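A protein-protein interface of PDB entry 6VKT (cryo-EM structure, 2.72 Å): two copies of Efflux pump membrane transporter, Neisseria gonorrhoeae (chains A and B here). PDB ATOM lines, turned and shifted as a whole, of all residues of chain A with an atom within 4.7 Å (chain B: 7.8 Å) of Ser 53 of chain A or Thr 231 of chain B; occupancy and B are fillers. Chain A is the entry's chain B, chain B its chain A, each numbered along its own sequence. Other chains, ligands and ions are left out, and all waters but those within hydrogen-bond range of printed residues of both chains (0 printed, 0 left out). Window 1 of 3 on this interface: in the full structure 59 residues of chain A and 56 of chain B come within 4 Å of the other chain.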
ATOM      1  N   GLY A  51      15.868 -13.493  13.731  1.00  0.00           N
ATOM      2  CA  GLY A  51      16.491 -14.526  12.930  1.00  0.00           C
ATOM      3  C   GLY A  51      15.640 -15.769  12.786  1.00  0.00           C
ATOM      4  O   GLY A  51      16.077 -16.868  13.138  1.00  0.00           O
ATOM      5  N   ALA A  52      14.425 -15.612  12.269  1.00  0.00           N
ATOM      6  CA  ALA A  52      13.532 -16.745  12.083  1.00  0.00           C
ATOM      7  C   ALA A  52      12.555 -16.427  10.963  1.00  0.00           C
ATOM      8  O   ALA A  52      12.268 -15.263  10.675  1.00  0.00           O
ATOM      9  CB  ALA A  52      12.781 -17.088  13.372  1.00  0.00           C
ATOM     10  N   SER A  53      12.045 -17.483  10.339  1.00  0.00           N
ATOM     11  CA  SER A  53      11.093 -17.350   9.248  1.00  0.00           C
ATOM     12  C   SER A  53       9.689 -17.157   9.819  1.00  0.00           C
ATOM     13  O   SER A  53       9.500 -17.017  11.030  1.00  0.00           O
ATOM     14  CB  SER A  53      11.176 -18.565   8.327  1.00  0.00           C
ATOM     15  OG  SER A  53      10.966 -19.766   9.046  1.00  0.00           O
ATOM     16  N   ALA A  54       8.684 -17.149   8.943  1.00  0.00           N
ATOM     17  CA  ALA A  54       7.312 -16.961   9.397  1.00  0.00           C
ATOM     18  C   ALA A  54       6.743 -18.234  10.010  1.00  0.00           C
ATOM     19  O   ALA A  54       6.063 -18.177  11.040  1.00  0.00           O
ATOM     20  CB  ALA A  54       6.436 -16.491   8.237  1.00  0.00           C
ATOM     21  N   GLN A  55       7.015 -19.389   9.398  1.00  0.00           N
ATOM     22  CA  GLN A  55       6.459 -20.641   9.903  1.00  0.00           C
ATOM     23  C   GLN A  55       7.038 -21.000  11.264  1.00  0.00           C
ATOM     24  O   GLN A  55       6.301 -21.406  12.170  1.00  0.00           O
ATOM     25  CB  GLN A  55       6.711 -21.767   8.901  1.00  0.00           C
ATOM     26  CG  GLN A  55       5.946 -21.623   7.598  1.00  0.00           C
ATOM     27  CD  GLN A  55       6.155 -22.802   6.672  1.00  0.00           C
ATOM     28  OE1 GLN A  55       7.105 -23.570   6.830  1.00  0.00           O
ATOM     29  NE2 GLN A  55       5.265 -22.957   5.698  1.00  0.00           N
ATOM     30  N   VAL A  56       8.357 -20.868  11.423  1.00  0.00           N
ATOM     31  CA  VAL A  56       8.994 -21.196  12.696  1.00  0.00           C
ATOM     32  C   VAL A  56       8.469 -20.288  13.800  1.00  0.00           C
ATOM     33  O   VAL A  56       8.048 -20.756  14.865  1.00  0.00           O
ATOM     34  CB  VAL A  56      10.525 -21.101  12.573  1.00  0.00           C
ATOM     35  CG1 VAL A  56      11.163 -21.036  13.950  1.00  0.00           C
ATOM     36  CG2 VAL A  56      11.066 -22.283  11.786  1.00  0.00           C
ATOM     37  N   MET A  57       8.482 -18.975  13.554  1.00  0.00           N
ATOM     38  CA  MET A  57       7.997 -18.016  14.541  1.00  0.00           C
ATOM     39  C   MET A  57       6.543 -18.289  14.902  1.00  0.00           C
ATOM     40  O   MET A  57       6.182 -18.325  16.086  1.00  0.00           O
ATOM     41  CB  MET A  57       8.160 -16.593  14.005  1.00  0.00           C
ATOM     42  CG  MET A  57       7.404 -15.534  14.789  1.00  0.00           C
ATOM     43  SD  MET A  57       8.030 -15.318  16.464  1.00  0.00           S
ATOM     44  CE  MET A  57       7.008 -13.964  17.032  1.00  0.00           C
ATOM     45  N   ASP A  83       5.831 -12.509   9.970  1.00  0.00           N
ATOM     46  CA  ASP A  83       6.556 -12.213   8.742  1.00  0.00           C
ATOM     47  C   ASP A  83       7.993 -12.695   8.906  1.00  0.00           C
ATOM     48  O   ASP A  83       8.347 -13.329   9.905  1.00  0.00           O
ATOM     49  CB  ASP A  83       6.477 -10.717   8.410  1.00  0.00           C
ATOM     50  CG  ASP A  83       6.748  -9.840   9.614  1.00  0.00           C
ATOM     51  OD1 ASP A  83       6.993 -10.391  10.707  1.00  0.00           O
ATOM     52  OD2 ASP A  83       6.714  -8.600   9.470  1.00  0.00           O
ATOM     53  N   SER A  84       8.828 -12.390   7.916  1.00  0.00           N
ATOM     54  CA  SER A  84      10.228 -12.792   7.922  1.00  0.00           C
ATOM     55  C   SER A  84      11.134 -11.777   8.602  1.00  0.00           C
ATOM     56  O   SER A  84      12.347 -11.997   8.668  1.00  0.00           O
ATOM     57  CB  SER A  84      10.712 -13.035   6.489  1.00  0.00           C
ATOM     58  OG  SER A  84      10.108 -14.190   5.935  1.00  0.00           O
ATOM     59  N   PRO A 722      11.769 -16.620  -3.154  1.00  0.00           N
ATOM     60  CA  PRO A 722      12.835 -17.627  -3.159  1.00  0.00           C
ATOM     61  C   PRO A 722      13.578 -17.643  -1.832  1.00  0.00           C
ATOM     62  O   PRO A 722      13.932 -16.598  -1.282  1.00  0.00           O
ATOM     63  CB  PRO A 722      13.742 -17.181  -4.311  1.00  0.00           C
ATOM     64  CG  PRO A 722      13.464 -15.725  -4.470  1.00  0.00           C
ATOM     65  CD  PRO A 722      12.015 -15.546  -4.131  1.00  0.00           C
ATOM     66  N   GLN A 723      13.809 -18.848  -1.319  1.00  0.00           N
ATOM     67  CA  GLN A 723      14.477 -19.058  -0.044  1.00  0.00           C
ATOM     68  C   GLN A 723      15.676 -19.975  -0.251  1.00  0.00           C
ATOM     69  O   GLN A 723      15.921 -20.476  -1.351  1.00  0.00           O
ATOM     70  CB  GLN A 723      13.510 -19.639   0.995  1.00  0.00           C
ATOM     71  CG  GLN A 723      12.382 -18.697   1.377  1.00  0.00           C
ATOM     72  CD  GLN A 723      11.483 -19.269   2.453  1.00  0.00           C
ATOM     73  OE1 GLN A 723      11.608 -20.435   2.826  1.00  0.00           O
ATOM     74  NE2 GLN A 723      10.568 -18.450   2.958  1.00  0.00           N
ATOM     75  N   LEU A 724      16.423 -20.199   0.826  1.00  0.00           N
ATOM     76  CA  LEU A 724      17.671 -20.955   0.801  1.00  0.00           C
ATOM     77  C   LEU A 724      17.646 -22.050   1.858  1.00  0.00           C
ATOM     78  O   LEU A 724      18.556 -22.178   2.680  1.00  0.00           O
ATOM     79  CB  LEU A 724      18.870 -20.034   1.003  1.00  0.00           C
ATOM     80  CG  LEU A 724      20.230 -20.600   0.591  1.00  0.00           C
ATOM     81  CD1 LEU A 724      20.237 -20.951  -0.888  1.00  0.00           C
ATOM     82  CD2 LEU A 724      21.341 -19.616   0.916  1.00  0.00           C
ATOM     83  N   GLU A 811       6.513 -15.824   2.813  1.00  0.00           N
ATOM     84  CA  GLU A 811       7.109 -14.718   3.548  1.00  0.00           C
ATOM     85  C   GLU A 811       6.161 -14.114   4.572  1.00  0.00           C
ATOM     86  O   GLU A 811       6.525 -13.134   5.231  1.00  0.00           O
ATOM     87  CB  GLU A 811       7.581 -13.631   2.577  1.00  0.00           C
ATOM     88  CG  GLU A 811       8.704 -14.069   1.652  1.00  0.00           C
ATOM     89  CD  GLU A 811      10.015 -14.277   2.383  1.00  0.00           C
ATOM     90  OE1 GLU A 811      10.270 -13.551   3.366  1.00  0.00           O
ATOM     91  OE2 GLU A 811      10.791 -15.168   1.978  1.00  0.00           O
ATOM     92  N   GLN B 211      14.517 -26.934  17.484  1.00  0.00           N
ATOM     93  CA  GLN B 211      14.239 -26.084  16.336  1.00  0.00           C
ATOM     94  C   GLN B 211      15.452 -25.226  16.000  1.00  0.00           C
ATOM     95  O   GLN B 211      16.168 -24.756  16.890  1.00  0.00           O
ATOM     96  CB  GLN B 211      13.028 -25.196  16.613  1.00  0.00           C
ATOM     97  CG  GLN B 211      12.400 -24.602  15.365  1.00  0.00           C
ATOM     98  CD  GLN B 211      11.055 -23.964  15.640  1.00  0.00           C
ATOM     99  OE1 GLN B 211      10.831 -23.398  16.711  1.00  0.00           O
ATOM    100  NE2 GLN B 211      10.149 -24.052  14.673  1.00  0.00           N
ATOM    101  N   ILE B 212      15.680 -25.020  14.706  1.00  0.00           N
ATOM    102  CA  ILE B 212      16.825 -24.267  14.208  1.00  0.00           C
ATOM    103  C   ILE B 212      16.320 -22.983  13.566  1.00  0.00           C
ATOM    104  O   ILE B 212      15.319 -22.996  12.838  1.00  0.00           O
ATOM    105  CB  ILE B 212      17.651 -25.091  13.207  1.00  0.00           C
ATOM    106  CG1 ILE B 212      18.076 -26.420  13.835  1.00  0.00           C
ATOM    107  CG2 ILE B 212      18.866 -24.305  12.745  1.00  0.00           C
ATOM    108  CD1 ILE B 212      18.831 -27.327  12.889  1.00  0.00           C
ATOM    109  N   SER B 213      17.013 -21.878  13.835  1.00  0.00           N
ATOM    110  CA  SER B 213      16.698 -20.575  13.256  1.00  0.00           C
ATOM    111  C   SER B 213      17.942 -20.068  12.539  1.00  0.00           C
ATOM    112  O   SER B 213      18.916 -19.665  13.184  1.00  0.00           O
ATOM    113  CB  SER B 213      16.242 -19.594  14.334  1.00  0.00           C
ATOM    114  OG  SER B 213      15.029 -20.021  14.930  1.00  0.00           O
ATOM    115  N   ALA B 214      17.910 -20.085  11.206  1.00  0.00           N
ATOM    116  CA  ALA B 214      19.095 -19.745  10.425  1.00  0.00           C
ATOM    117  C   ALA B 214      19.280 -18.235  10.315  1.00  0.00           C
ATOM    118  O   ALA B 214      20.287 -17.687  10.776  1.00  0.00           O
ATOM    119  CB  ALA B 214      19.006 -20.381   9.035  1.00  0.00           C
ATOM    120  N   GLY B 215      18.318 -17.547   9.707  1.00  0.00           N
ATOM    121  CA  GLY B 215      18.427 -16.115   9.513  1.00  0.00           C
ATOM    122  C   GLY B 215      18.184 -15.688   8.081  1.00  0.00           C
ATOM    123  O   GLY B 215      17.319 -16.244   7.399  1.00  0.00           O
ATOM    124  N   SER B 216      18.951 -14.711   7.603  1.00  0.00           N
ATOM    125  CA  SER B 216      18.745 -14.178   6.263  1.00  0.00           C
ATOM    126  C   SER B 216      20.087 -13.918   5.600  1.00  0.00           C
ATOM    127  O   SER B 216      20.938 -13.225   6.165  1.00  0.00           O
ATOM    128  CB  SER B 216      17.920 -12.887   6.306  1.00  0.00           C
ATOM    129  OG  SER B 216      16.618 -13.129   6.806  1.00  0.00           O
ATOM    130  N   ILE B 217      20.269 -14.479   4.409  1.00  0.00           N
ATOM    131  CA  ILE B 217      21.418 -14.160   3.570  1.00  0.00           C
ATOM    132  C   ILE B 217      21.147 -12.825   2.892  1.00  0.00           C
ATOM    133  O   ILE B 217      20.099 -12.637   2.262  1.00  0.00           O
ATOM    134  CB  ILE B 217      21.674 -15.267   2.538  1.00  0.00           C
ATOM    135  CG1 ILE B 217      22.408 -16.442   3.186  1.00  0.00           C
ATOM    136  CG2 ILE B 217      22.465 -14.727   1.359  1.00  0.00           C
ATOM    137  CD1 ILE B 217      23.829 -16.121   3.594  1.00  0.00           C
ATOM    138  N   GLY B 218      22.087 -11.894   3.024  1.00  0.00           N
ATOM    139  CA  GLY B 218      21.884 -10.550   2.529  1.00  0.00           C
ATOM    140  C   GLY B 218      21.070  -9.716   3.496  1.00  0.00           C
ATOM    141  O   GLY B 218      20.087  -9.078   3.108  1.00  0.00           O
ATOM    142  N   THR B 229      18.091 -10.763  -1.155  1.00  0.00           N
ATOM    143  CA  THR B 229      17.977 -11.179   0.236  1.00  0.00           C
ATOM    144  C   THR B 229      17.108 -12.427   0.289  1.00  0.00           C
ATOM    145  O   THR B 229      16.060 -12.479  -0.363  1.00  0.00           O
ATOM    146  CB  THR B 229      17.368 -10.073   1.104  1.00  0.00           C
ATOM    147  OG1 THR B 229      18.086  -8.850   0.895  1.00  0.00           O
ATOM    148  CG2 THR B 229      17.437 -10.451   2.574  1.00  0.00           C
ATOM    149  N   ALA B 230      17.535 -13.426   1.058  1.00  0.00           N
ATOM    150  CA  ALA B 230      16.823 -14.697   1.094  1.00  0.00           C
ATOM    151  C   ALA B 230      16.792 -15.249   2.509  1.00  0.00           C
ATOM    152  O   ALA B 230      17.832 -15.339   3.166  1.00  0.00           O
ATOM    153  CB  ALA B 230      17.470 -15.716   0.148  1.00  0.00           C
ATOM    154  N   THR B 231      15.606 -15.637   2.968  1.00  0.00           N
ATOM    155  CA  THR B 231      15.462 -16.239   4.286  1.00  0.00           C
ATOM    156  C   THR B 231      15.945 -17.684   4.252  1.00  0.00           C
ATOM    157  O   THR B 231      15.489 -18.480   3.426  1.00  0.00           O
ATOM    158  CB  THR B 231      14.006 -16.182   4.745  1.00  0.00           C
ATOM    159  OG1 THR B 231      13.594 -14.815   4.866  1.00  0.00           O
ATOM    160  CG2 THR B 231      13.841 -16.877   6.087  1.00  0.00           C
ATOM    161  N   VAL B 232      16.870 -18.021   5.147  1.00  0.00           N
ATOM    162  CA  VAL B 232      17.416 -19.370   5.234  1.00  0.00           C
ATOM    163  C   VAL B 232      16.613 -20.154   6.261  1.00  0.00           C
ATOM    164  O   VAL B 232      16.369 -19.672   7.374  1.00  0.00           O
ATOM    165  CB  VAL B 232      18.907 -19.339   5.607  1.00  0.00           C
ATOM    166  CG1 VAL B 232      19.469 -20.749   5.659  1.00  0.00           C
ATOM    167  CG2 VAL B 232      19.683 -18.484   4.618  1.00  0.00           C
ATOM    168  N   THR B 233      16.198 -21.363   5.891  1.00  0.00           N
ATOM    169  CA  THR B 233      15.378 -22.203   6.751  1.00  0.00           C
ATOM    170  C   THR B 233      15.974 -23.600   6.835  1.00  0.00           C
ATOM    171  O   THR B 233      16.444 -24.148   5.834  1.00  0.00           O
ATOM    172  CB  THR B 233      13.933 -22.292   6.241  1.00  0.00           C
ATOM    173  OG1 THR B 233      13.862 -23.233   5.163  1.00  0.00           O
ATOM    174  CG2 THR B 233      13.451 -20.935   5.755  1.00  0.00           C
ATOM    175  N   ALA B 234      15.953 -24.168   8.039  1.00  0.00           N
ATOM    176  CA  ALA B 234      16.388 -25.537   8.283  1.00  0.00           C
ATOM    177  C   ALA B 234      15.420 -26.179   9.264  1.00  0.00           C
ATOM    178  O   ALA B 234      15.069 -25.569  10.279  1.00  0.00           O
ATOM    179  CB  ALA B 234      17.816 -25.580   8.834  1.00  0.00           C
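The backbone carbonyl oxygen (O) of Thr 231 of chain B lies within hydrogen-bond range of the backbone NH (N) of Leu 724 of chain A (3.3 Å).
The backbone NH (N) of Val 232 of chain B is in hydrogen-bond range of the backbone carbonyl oxygen (O) of Gly 215 of chain B, 2.9 Å away.
N of Ile 217 of chain B is in hydrogen-bond range of O of Ala 230 of chain B, at 2.9 Å.
The side-chain carboxylate of Glu 811 of chain A lies within hydrogen-bond range of the side-chain hydroxyl of Ser 84 of chain A.
The side-chain carboxylate (OE2) of Glu 811 of chain A is in hydrogen-bond range of the side-chain amide nitrogen (NE2) of Gln 723 of chain A (3.4 Å).
Among the printed residues, pairs that only touch across the chains: Gly 51 of chain A with Ser 213 of chain B (3.0 Å), Val 56 of chain A with Gln 211 of chain B (3.3 Å), Gln 723 of chain A with Thr 231 of chain B (3.3 Å), Leu 724 of chain A with Val 232 of chain B (3.4 Å), Gln 723 of chain A with Thr 233 of chain B (3.5 Å), Ser 84 of chain A with Thr 231 of chain B (3.7 Å), Glu 811 of chain A with Thr 231 of chain B (3.9 Å), Ser 53 of chain A with Thr 231 of chain B (3.9 Å) and Pro 722 of chain A with Ala 230 of chain B (3.9 Å).
Printed residues of chain B within 4 Å of Ser 53 of chain A: Thr 231 (3.9 Å).
Printed residues of chain B within 4 Å of Val 56 of chain A: Gln 211 (3.3 Å).
Asp 83 of chain A touches none of the printed residues of chain B.
Of the printed residues of chain B, Ser 84 of chain A touches Thr 231.
Printed residues of chain A within 4 Å of Gln 211 of chain B: Val 56.
Gly 215 of chain B touches none of the printed residues of chain A.
Thr 231 of chain B touches just these residues of chain A: Ser 53, Ser 84, Gln 723, Leu 724 and Glu 811.
Of the printed residues of chain A, Val 232 of chain B touches Leu 724 (3.4 Å).
The nearest printed residue of chain A that does not touch Thr 231 of chain B is Pro 722 of chain A (4.7 Å).
The nearest printed residue of chain B that does not touch Leu 724 of chain A is Ile 217 of chain B (4.05 Å).
Hydrophobic or aromatic side chains of chain B within 4 Å of the printed part of chain A: Ala 230 and Val 232.
Hydrophobic or aromatic side chains of chain A that line the printed part of chain B: Val 56.
No position is printed for both chains.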
